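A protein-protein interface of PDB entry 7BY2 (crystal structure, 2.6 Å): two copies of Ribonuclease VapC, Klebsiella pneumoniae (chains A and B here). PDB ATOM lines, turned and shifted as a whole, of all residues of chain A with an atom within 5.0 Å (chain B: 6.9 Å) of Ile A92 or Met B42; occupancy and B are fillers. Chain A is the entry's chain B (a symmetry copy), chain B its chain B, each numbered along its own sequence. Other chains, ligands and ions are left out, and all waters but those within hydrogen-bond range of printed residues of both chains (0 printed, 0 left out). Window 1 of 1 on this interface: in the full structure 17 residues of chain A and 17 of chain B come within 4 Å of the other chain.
Ile A69 touches Leu B38.
Leu B38 touches Ala A74 (CD1 to CB, 3.96 Å).
Met B42 touches Ala A74.
Val A78 touches Met B42.
CG1 of Val A78 touches O of Met B45, 3.996 Å away.
CD1 of Ile A92 touches CE of Met B42 (3.7 Å).
OG1 of Thr A96 is in hydrogen-bond range of O of Ile A92 (2.6 Å).
Hydrophobic or aromatic side chains of chain A that line the printed part of chain B: Ile A69, Ala A74, Val A78 and Ile A92.
Printed residues of chain B that touch a printed residue of chain A: Leu B38, Met B42 and Met B45.
Along chain B the printed residues that touch a printed residue of chain A span positions 38 to 45.
Of the printed residues of chain B, Val A78 touches Met B42 and Met B45.
Asp A90 touches none of the printed residues of chain B.
Printed residues of chain A within 4 Å of Leu B38: Ile A69 and Ala A74.
Printed residues of chain A within 4 Å of Met B42: Ala A74, Val A78 and Ile A92.
Of the printed residues of chain A, Met B45 touches Val A78.
The nearest residue of chain B that does not touch Ile A92 is Ile B39 (6.0 Å).
The nearest printed residue of chain B that does not touch Ile A69 is Ile B69 (4.1 Å).
3 positions are printed for both chains.
Of the 6 pairs that touch across the chains among the printed residues, none has its exchanged pair printed and touching as well.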
ATOM      1  N   SER A  37     -30.431 -38.616 -17.275  1.00  0.00           N
ATOM      2  CA  SER A  37     -30.057 -37.392 -17.972  1.00  0.00           C
ATOM      3  C   SER A  37     -29.023 -37.703 -19.046  1.00  0.00           C
ATOM      4  O   SER A  37     -28.305 -38.699 -18.954  1.00  0.00           O
ATOM      5  CB  SER A  37     -29.511 -36.353 -16.992  1.00  0.00           C
ATOM      6  OG  SER A  37     -28.949 -35.247 -17.682  1.00  0.00           O
ATOM      7  N   ILE A  39     -26.453 -36.096 -19.449  1.00  0.00           N
ATOM      8  CA  ILE A  39     -25.200 -35.945 -18.718  1.00  0.00           C
ATOM      9  C   ILE A  39     -24.737 -37.284 -18.156  1.00  0.00           C
ATOM     10  O   ILE A  39     -23.585 -37.679 -18.342  1.00  0.00           O
ATOM     11  CB  ILE A  39     -25.342 -34.931 -17.567  1.00  0.00           C
ATOM     12  CG1 ILE A  39     -25.334 -33.505 -18.114  1.00  0.00           C
ATOM     13  CG2 ILE A  39     -24.215 -35.098 -16.561  1.00  0.00           C
ATOM     14  CD1 ILE A  39     -25.525 -32.457 -17.051  1.00  0.00           C
ATOM     15  N   ILE A  69     -31.247 -31.877 -22.609  1.00  0.00           N
ATOM     16  CA  ILE A  69     -31.440 -30.674 -21.821  1.00  0.00           C
ATOM     17  C   ILE A  69     -32.233 -29.650 -22.617  1.00  0.00           C
ATOM     18  O   ILE A  69     -31.728 -29.067 -23.575  1.00  0.00           O
ATOM     19  CB  ILE A  69     -30.087 -30.068 -21.398  1.00  0.00           C
ATOM     20  CG1 ILE A  69     -29.207 -31.139 -20.746  1.00  0.00           C
ATOM     21  CG2 ILE A  69     -30.294 -28.878 -20.468  1.00  0.00           C
ATOM     22  CD1 ILE A  69     -27.814 -30.662 -20.410  1.00  0.00           C
ATOM     23  N   ILE A  73     -35.116 -27.036 -18.630  1.00  0.00           N
ATOM     24  CA  ILE A  73     -34.164 -27.657 -17.721  1.00  0.00           C
ATOM     25  C   ILE A  73     -32.984 -26.724 -17.464  1.00  0.00           C
ATOM     26  O   ILE A  73     -32.456 -26.668 -16.353  1.00  0.00           O
ATOM     27  CB  ILE A  73     -33.674 -29.009 -18.284  1.00  0.00           C
ATOM     28  CG1 ILE A  73     -34.828 -30.014 -18.304  1.00  0.00           C
ATOM     29  CG2 ILE A  73     -32.523 -29.561 -17.463  1.00  0.00           C
ATOM     30  CD1 ILE A  73     -34.526 -31.284 -19.061  1.00  0.00           C
ATOM     31  N   ALA A  74     -32.589 -25.979 -18.492  1.00  0.00           N
ATOM     32  CA  ALA A  74     -31.504 -25.014 -18.360  1.00  0.00           C
ATOM     33  C   ALA A  74     -31.871 -23.907 -17.374  1.00  0.00           C
ATOM     34  O   ALA A  74     -31.064 -23.536 -16.523  1.00  0.00           O
ATOM     35  CB  ALA A  74     -31.152 -24.421 -19.715  1.00  0.00           C
ATOM     36  N   SER A  77     -32.109 -25.472 -13.764  1.00  0.00           N
ATOM     37  CA  SER A  77     -30.785 -25.827 -13.261  1.00  0.00           C
ATOM     38  C   SER A  77     -30.095 -24.619 -12.636  1.00  0.00           C
ATOM     39  O   SER A  77     -29.516 -24.715 -11.553  1.00  0.00           O
ATOM     40  CB  SER A  77     -29.919 -26.399 -14.385  1.00  0.00           C
ATOM     41  OG  SER A  77     -30.606 -27.416 -15.089  1.00  0.00           O
ATOM     42  N   VAL A  78     -30.167 -23.487 -13.329  1.00  0.00           N
ATOM     43  CA  VAL A  78     -29.581 -22.240 -12.854  1.00  0.00           C
ATOM     44  C   VAL A  78     -30.168 -21.835 -11.505  1.00  0.00           C
ATOM     45  O   VAL A  78     -29.438 -21.482 -10.578  1.00  0.00           O
ATOM     46  CB  VAL A  78     -29.798 -21.097 -13.867  1.00  0.00           C
ATOM     47  CG1 VAL A  78     -29.384 -19.760 -13.271  1.00  0.00           C
ATOM     48  CG2 VAL A  78     -29.032 -21.376 -15.153  1.00  0.00           C
ATOM     49  N   LEU A  88     -23.210 -27.683 -10.676  1.00  0.00           N
ATOM     50  CA  LEU A  88     -24.126 -27.522 -11.806  1.00  0.00           C
ATOM     51  C   LEU A  88     -24.633 -28.835 -12.432  1.00  0.00           C
ATOM     52  O   LEU A  88     -25.826 -28.943 -12.719  1.00  0.00           O
ATOM     53  CB  LEU A  88     -23.477 -26.658 -12.892  1.00  0.00           C
ATOM     54  CG  LEU A  88     -24.385 -26.325 -14.078  1.00  0.00           C
ATOM     55  CD1 LEU A  88     -25.654 -25.631 -13.601  1.00  0.00           C
ATOM     56  CD2 LEU A  88     -23.653 -25.463 -15.094  1.00  0.00           C
ATOM     57  N   PRO A  89     -23.748 -29.829 -12.655  1.00  0.00           N
ATOM     58  CA  PRO A  89     -24.297 -31.076 -13.202  1.00  0.00           C
ATOM     59  C   PRO A  89     -25.282 -31.761 -12.255  1.00  0.00           C
ATOM     60  O   PRO A  89     -26.175 -32.472 -12.717  1.00  0.00           O
ATOM     61  CB  PRO A  89     -23.054 -31.949 -13.421  1.00  0.00           C
ATOM     62  CG  PRO A  89     -22.001 -31.352 -12.554  1.00  0.00           C
ATOM     63  CD  PRO A  89     -22.278 -29.885 -12.553  1.00  0.00           C
ATOM     64  N   ASP A  90     -25.120 -31.549 -10.952  1.00  0.00           N
ATOM     65  CA  ASP A  90     -26.095 -32.033  -9.982  1.00  0.00           C
ATOM     66  C   ASP A  90     -27.418 -31.302 -10.183  1.00  0.00           C
ATOM     67  O   ASP A  90     -28.491 -31.904 -10.120  1.00  0.00           O
ATOM     68  CB  ASP A  90     -25.599 -31.828  -8.548  1.00  0.00           C
ATOM     69  CG  ASP A  90     -24.317 -32.581  -8.261  1.00  0.00           C
ATOM     70  OD1 ASP A  90     -24.124 -33.671  -8.835  1.00  0.00           O
ATOM     71  OD2 ASP A  90     -23.502 -32.079  -7.456  1.00  0.00           O
ATOM     72  N   ALA A  91     -27.324 -30.000 -10.429  1.00  0.00           N
ATOM     73  CA  ALA A  91     -28.498 -29.153 -10.591  1.00  0.00           C
ATOM     74  C   ALA A  91     -29.280 -29.506 -11.852  1.00  0.00           C
ATOM     75  O   ALA A  91     -30.510 -29.510 -11.843  1.00  0.00           O
ATOM     76  CB  ALA A  91     -28.090 -27.687 -10.616  1.00  0.00           C
ATOM     77  N   ILE A  92     -28.560 -29.800 -12.930  1.00  0.00           N
ATOM     78  CA  ILE A  92     -29.187 -30.148 -14.201  1.00  0.00           C
ATOM     79  C   ILE A  92     -29.979 -31.445 -14.082  1.00  0.00           C
ATOM     80  O   ILE A  92     -31.094 -31.556 -14.593  1.00  0.00           O
ATOM     81  CB  ILE A  92     -28.139 -30.280 -15.325  1.00  0.00           C
ATOM     82  CG1 ILE A  92     -27.456 -28.934 -15.568  1.00  0.00           C
ATOM     83  CG2 ILE A  92     -28.784 -30.782 -16.607  1.00  0.00           C
ATOM     84  CD1 ILE A  92     -26.275 -29.006 -16.506  1.00  0.00           C
ATOM     85  N   ILE A  93     -29.398 -32.421 -13.394  1.00  0.00           N
ATOM     86  CA  ILE A  93     -30.046 -33.711 -13.194  1.00  0.00           C
ATOM     87  C   ILE A  93     -31.263 -33.565 -12.280  1.00  0.00           C
ATOM     88  O   ILE A  93     -32.308 -34.172 -12.523  1.00  0.00           O
ATOM     89  CB  ILE A  93     -29.060 -34.744 -12.611  1.00  0.00           C
ATOM     90  CG1 ILE A  93     -27.986 -35.085 -13.647  1.00  0.00           C
ATOM     91  CG2 ILE A  93     -29.782 -36.008 -12.193  1.00  0.00           C
ATOM     92  CD1 ILE A  93     -26.821 -35.871 -13.087  1.00  0.00           C
ATOM     93  N   LEU A  94     -31.127 -32.749 -11.239  1.00  0.00           N
ATOM     94  CA  LEU A  94     -32.245 -32.457 -10.345  1.00  0.00           C
ATOM     95  C   LEU A  94     -33.343 -31.701 -11.087  1.00  0.00           C
ATOM     96  O   LEU A  94     -34.531 -31.948 -10.876  1.00  0.00           O
ATOM     97  CB  LEU A  94     -31.774 -31.647  -9.134  1.00  0.00           C
ATOM     98  CG  LEU A  94     -32.855 -31.244  -8.125  1.00  0.00           C
ATOM     99  CD1 LEU A  94     -33.624 -32.466  -7.634  1.00  0.00           C
ATOM    100  CD2 LEU A  94     -32.251 -30.480  -6.956  1.00  0.00           C
ATOM    101  N   ALA A  95     -32.935 -30.781 -11.956  1.00  0.00           N
ATOM    102  CA  ALA A  95     -33.874 -30.018 -12.770  1.00  0.00           C
ATOM    103  C   ALA A  95     -34.603 -30.932 -13.744  1.00  0.00           C
ATOM    104  O   ALA A  95     -35.803 -30.778 -13.978  1.00  0.00           O
ATOM    105  CB  ALA A  95     -33.151 -28.913 -13.521  1.00  0.00           C
ATOM    106  N   THR A  96     -33.865 -31.881 -14.307  1.00  0.00           N
ATOM    107  CA  THR A  96     -34.427 -32.854 -15.236  1.00  0.00           C
ATOM    108  C   THR A  96     -35.506 -33.688 -14.556  1.00  0.00           C
ATOM    109  O   THR A  96     -36.562 -33.949 -15.135  1.00  0.00           O
ATOM    110  CB  THR A  96     -33.337 -33.787 -15.794  1.00  0.00           C
ATOM    111  OG1 THR A  96     -32.297 -33.006 -16.394  1.00  0.00           O
ATOM    112  CG2 THR A  96     -33.920 -34.729 -16.834  1.00  0.00           C
ATOM    113  N   ILE B  36     -22.772 -19.862 -28.893  1.00  0.00           N
ATOM    114  CA  ILE B  36     -22.293 -20.378 -27.615  1.00  0.00           C
ATOM    115  C   ILE B  36     -22.993 -21.693 -27.295  1.00  0.00           C
ATOM    116  O   ILE B  36     -24.099 -21.949 -27.774  1.00  0.00           O
ATOM    117  CB  ILE B  36     -22.535 -19.392 -26.451  1.00  0.00           C
ATOM    118  CG1 ILE B  36     -24.030 -19.095 -26.300  1.00  0.00           C
ATOM    119  CG2 ILE B  36     -21.743 -18.108 -26.650  1.00  0.00           C
ATOM    120  CD1 ILE B  36     -24.375 -18.337 -25.037  1.00  0.00           C
ATOM    121  N   SER B  37     -22.348 -22.526 -26.488  1.00  0.00           N
ATOM    122  CA  SER B  37     -22.969 -23.760 -26.028  1.00  0.00           C
ATOM    123  C   SER B  37     -24.014 -23.451 -24.965  1.00  0.00           C
ATOM    124  O   SER B  37     -23.943 -22.417 -24.300  1.00  0.00           O
ATOM    125  CB  SER B  37     -21.918 -24.726 -25.476  1.00  0.00           C
ATOM    126  OG  SER B  37     -22.530 -25.833 -24.835  1.00  0.00           O
ATOM    127  N   LEU B  38     -24.985 -24.346 -24.812  1.00  0.00           N
ATOM    128  CA  LEU B  38     -26.006 -24.200 -23.780  1.00  0.00           C
ATOM    129  C   LEU B  38     -25.361 -24.245 -22.398  1.00  0.00           C
ATOM    130  O   LEU B  38     -25.868 -23.657 -21.442  1.00  0.00           O
ATOM    131  CB  LEU B  38     -27.072 -25.291 -23.916  1.00  0.00           C
ATOM    132  CG  LEU B  38     -28.241 -25.268 -22.929  1.00  0.00           C
ATOM    133  CD1 LEU B  38     -28.959 -23.929 -22.973  1.00  0.00           C
ATOM    134  CD2 LEU B  38     -29.209 -26.407 -23.215  1.00  0.00           C
ATOM    135  N   ILE B  39     -24.235 -24.947 -22.308  1.00  0.00           N
ATOM    136  CA  ILE B  39     -23.447 -25.003 -21.082  1.00  0.00           C
ATOM    137  C   ILE B  39     -22.933 -23.618 -20.706  1.00  0.00           C
ATOM    138  O   ILE B  39     -23.091 -23.175 -19.567  1.00  0.00           O
ATOM    139  CB  ILE B  39     -22.254 -25.967 -21.224  1.00  0.00           C
ATOM    140  CG1 ILE B  39     -22.730 -27.414 -21.126  1.00  0.00           C
ATOM    141  CG2 ILE B  39     -21.213 -25.699 -20.151  1.00  0.00           C
ATOM    142  CD1 ILE B  39     -21.626 -28.420 -21.313  1.00  0.00           C
ATOM    143  N   THR B  40     -22.318 -22.943 -21.673  1.00  0.00           N
ATOM    144  CA  THR B  40     -21.813 -21.589 -21.477  1.00  0.00           C
ATOM    145  C   THR B  40     -22.946 -20.658 -21.053  1.00  0.00           C
ATOM    146  O   THR B  40     -22.764 -19.793 -20.197  1.00  0.00           O
ATOM    147  CB  THR B  40     -21.140 -21.050 -22.757  1.00  0.00           C
ATOM    148  OG1 THR B  40     -19.935 -21.783 -23.008  1.00  0.00           O
ATOM    149  CG2 THR B  40     -20.802 -19.573 -22.614  1.00  0.00           C
ATOM    150  N   TRP B  41     -24.118 -20.858 -21.648  1.00  0.00           N
ATOM    151  CA  TRP B  41     -25.302 -20.081 -21.298  1.00  0.00           C
ATOM    152  C   TRP B  41     -25.640 -20.239 -19.820  1.00  0.00           C
ATOM    153  O   TRP B  41     -25.875 -19.257 -19.121  1.00  0.00           O
ATOM    154  CB  TRP B  41     -26.495 -20.503 -22.157  1.00  0.00           C
ATOM    155  CG  TRP B  41     -27.694 -19.621 -21.998  1.00  0.00           C
ATOM    156  CD1 TRP B  41     -28.019 -18.535 -22.759  1.00  0.00           C
ATOM    157  CD2 TRP B  41     -28.736 -19.739 -21.017  1.00  0.00           C
ATOM    158  NE1 TRP B  41     -29.191 -17.974 -22.315  1.00  0.00           N
ATOM    159  CE2 TRP B  41     -29.649 -18.699 -21.244  1.00  0.00           C
ATOM    160  CE3 TRP B  41     -28.974 -20.636 -19.966  1.00  0.00           C
ATOM    161  CZ2 TRP B  41     -30.791 -18.519 -20.464  1.00  0.00           C
ATOM    162  CZ3 TRP B  41     -30.108 -20.455 -19.192  1.00  0.00           C
ATOM    163  CH2 TRP B  41     -31.001 -19.407 -19.444  1.00  0.00           C
ATOM    164  N   MET B  42     -25.654 -21.483 -19.350  1.00  0.00           N
ATOM    165  CA  MET B  42     -25.959 -21.772 -17.954  1.00  0.00           C
ATOM    166  C   MET B  42     -24.893 -21.217 -17.016  1.00  0.00           C
ATOM    167  O   MET B  42     -25.213 -20.617 -15.990  1.00  0.00           O
ATOM    168  CB  MET B  42     -26.111 -23.281 -17.739  1.00  0.00           C
ATOM    169  CG  MET B  42     -27.447 -23.843 -18.203  1.00  0.00           C
ATOM    170  SD  MET B  42     -27.609 -25.760 -17.879  1.00  0.00           S
ATOM    171  CE  MET B  42     -26.232 -26.391 -19.107  1.00  0.00           C
ATOM    172  N   GLU B  43     -23.627 -21.419 -17.372  1.00  0.00           N
ATOM    173  CA  GLU B  43     -22.512 -20.947 -16.556  1.00  0.00           C
ATOM    174  C   GLU B  43     -22.527 -19.427 -16.410  1.00  0.00           C
ATOM    175  O   GLU B  43     -22.250 -18.895 -15.336  1.00  0.00           O
ATOM    176  CB  GLU B  43     -21.179 -21.405 -17.155  1.00  0.00           C
ATOM    177  CG  GLU B  43     -20.959 -22.911 -17.105  1.00  0.00           C
ATOM    178  CD  GLU B  43     -19.661 -23.333 -17.768  1.00  0.00           C
ATOM    179  OE1 GLU B  43     -19.028 -22.486 -18.430  1.00  0.00           O
ATOM    180  OE2 GLU B  43     -19.272 -24.511 -17.629  1.00  0.00           O
ATOM    181  N   VAL B  44     -22.855 -18.733 -17.497  1.00  0.00           N
ATOM    182  CA  VAL B  44     -22.927 -17.277 -17.484  1.00  0.00           C
ATOM    183  C   VAL B  44     -24.147 -16.792 -16.703  1.00  0.00           C
ATOM    184  O   VAL B  44     -24.047 -15.870 -15.892  1.00  0.00           O
ATOM    185  CB  VAL B  44     -22.969 -16.702 -18.918  1.00  0.00           C
ATOM    186  CG1 VAL B  44     -23.378 -15.237 -18.903  1.00  0.00           C
ATOM    187  CG2 VAL B  44     -21.618 -16.873 -19.597  1.00  0.00           C
ATOM    188  N   MET B  45     -25.294 -17.423 -16.942  1.00  0.00           N
ATOM    189  CA  MET B  45     -26.534 -17.040 -16.273  1.00  0.00           C
ATOM    190  C   MET B  45     -26.453 -17.224 -14.758  1.00  0.00           C
ATOM    191  O   MET B  45     -27.144 -16.534 -14.010  1.00  0.00           O
ATOM    192  CB  MET B  45     -27.717 -17.834 -16.831  1.00  0.00           C
ATOM    193  CG  MET B  45     -28.227 -17.322 -18.168  1.00  0.00           C
ATOM    194  SD  MET B  45     -28.694 -15.429 -18.112  1.00  0.00           S
ATOM    195  CE  MET B  45     -30.061 -15.491 -16.724  1.00  0.00           C
ATOM    196  N   VAL B  46     -25.615 -18.157 -14.314  1.00  0.00           N
ATOM    197  CA  VAL B  46     -25.367 -18.341 -12.889  1.00  0.00           C
ATOM    198  C   VAL B  46     -24.733 -17.079 -12.309  1.00  0.00           C
ATOM    199  O   VAL B  46     -25.122 -16.610 -11.237  1.00  0.00           O
ATOM    200  CB  VAL B  46     -24.454 -19.558 -12.619  1.00  0.00           C
ATOM    201  CG1 VAL B  46     -23.844 -19.482 -11.227  1.00  0.00           C
ATOM    202  CG2 VAL B  46     -25.230 -20.854 -12.797  1.00  0.00           C
ATOM    203  N   GLY B  47     -23.770 -16.525 -13.036  1.00  0.00           N
ATOM    204  CA  GLY B  47     -23.110 -15.300 -12.624  1.00  0.00           C
ATOM    205  C   GLY B  47     -24.044 -14.105 -12.648  1.00  0.00           C
ATOM    206  O   GLY B  47     -23.910 -13.188 -11.838  1.00  0.00           O
ATOM    207  N   LEU B  61     -27.337 -12.494 -24.170  1.00  0.00           N
ATOM    208  CA  LEU B  61     -27.031 -13.864 -24.570  1.00  0.00           C
ATOM    209  C   LEU B  61     -27.927 -14.336 -25.711  1.00  0.00           C
ATOM    210  O   LEU B  61     -27.519 -15.162 -26.528  1.00  0.00           O
ATOM    211  CB  LEU B  61     -27.169 -14.815 -23.379  1.00  0.00           C
ATOM    212  CG  LEU B  61     -26.117 -14.716 -22.272  1.00  0.00           C
ATOM    213  CD1 LEU B  61     -26.391 -15.739 -21.179  1.00  0.00           C
ATOM    214  CD2 LEU B  61     -24.722 -14.899 -22.843  1.00  0.00           C
ATOM    215  N   ILE B  69     -27.375 -29.538 -26.760  1.00  0.00           N
ATOM    216  CA  ILE B  69     -26.537 -30.711 -26.929  1.00  0.00           C
ATOM    217  C   ILE B  69     -27.314 -31.809 -27.639  1.00  0.00           C
ATOM    218  O   ILE B  69     -28.221 -32.411 -27.067  1.00  0.00           O
ATOM    219  CB  ILE B  69     -26.031 -31.230 -25.569  1.00  0.00           C
ATOM    220  CG1 ILE B  69     -25.397 -30.089 -24.768  1.00  0.00           C
ATOM    221  CG2 ILE B  69     -25.053 -32.384 -25.759  1.00  0.00           C
ATOM    222  CD1 ILE B  69     -24.982 -30.480 -23.370  1.00  0.00           C
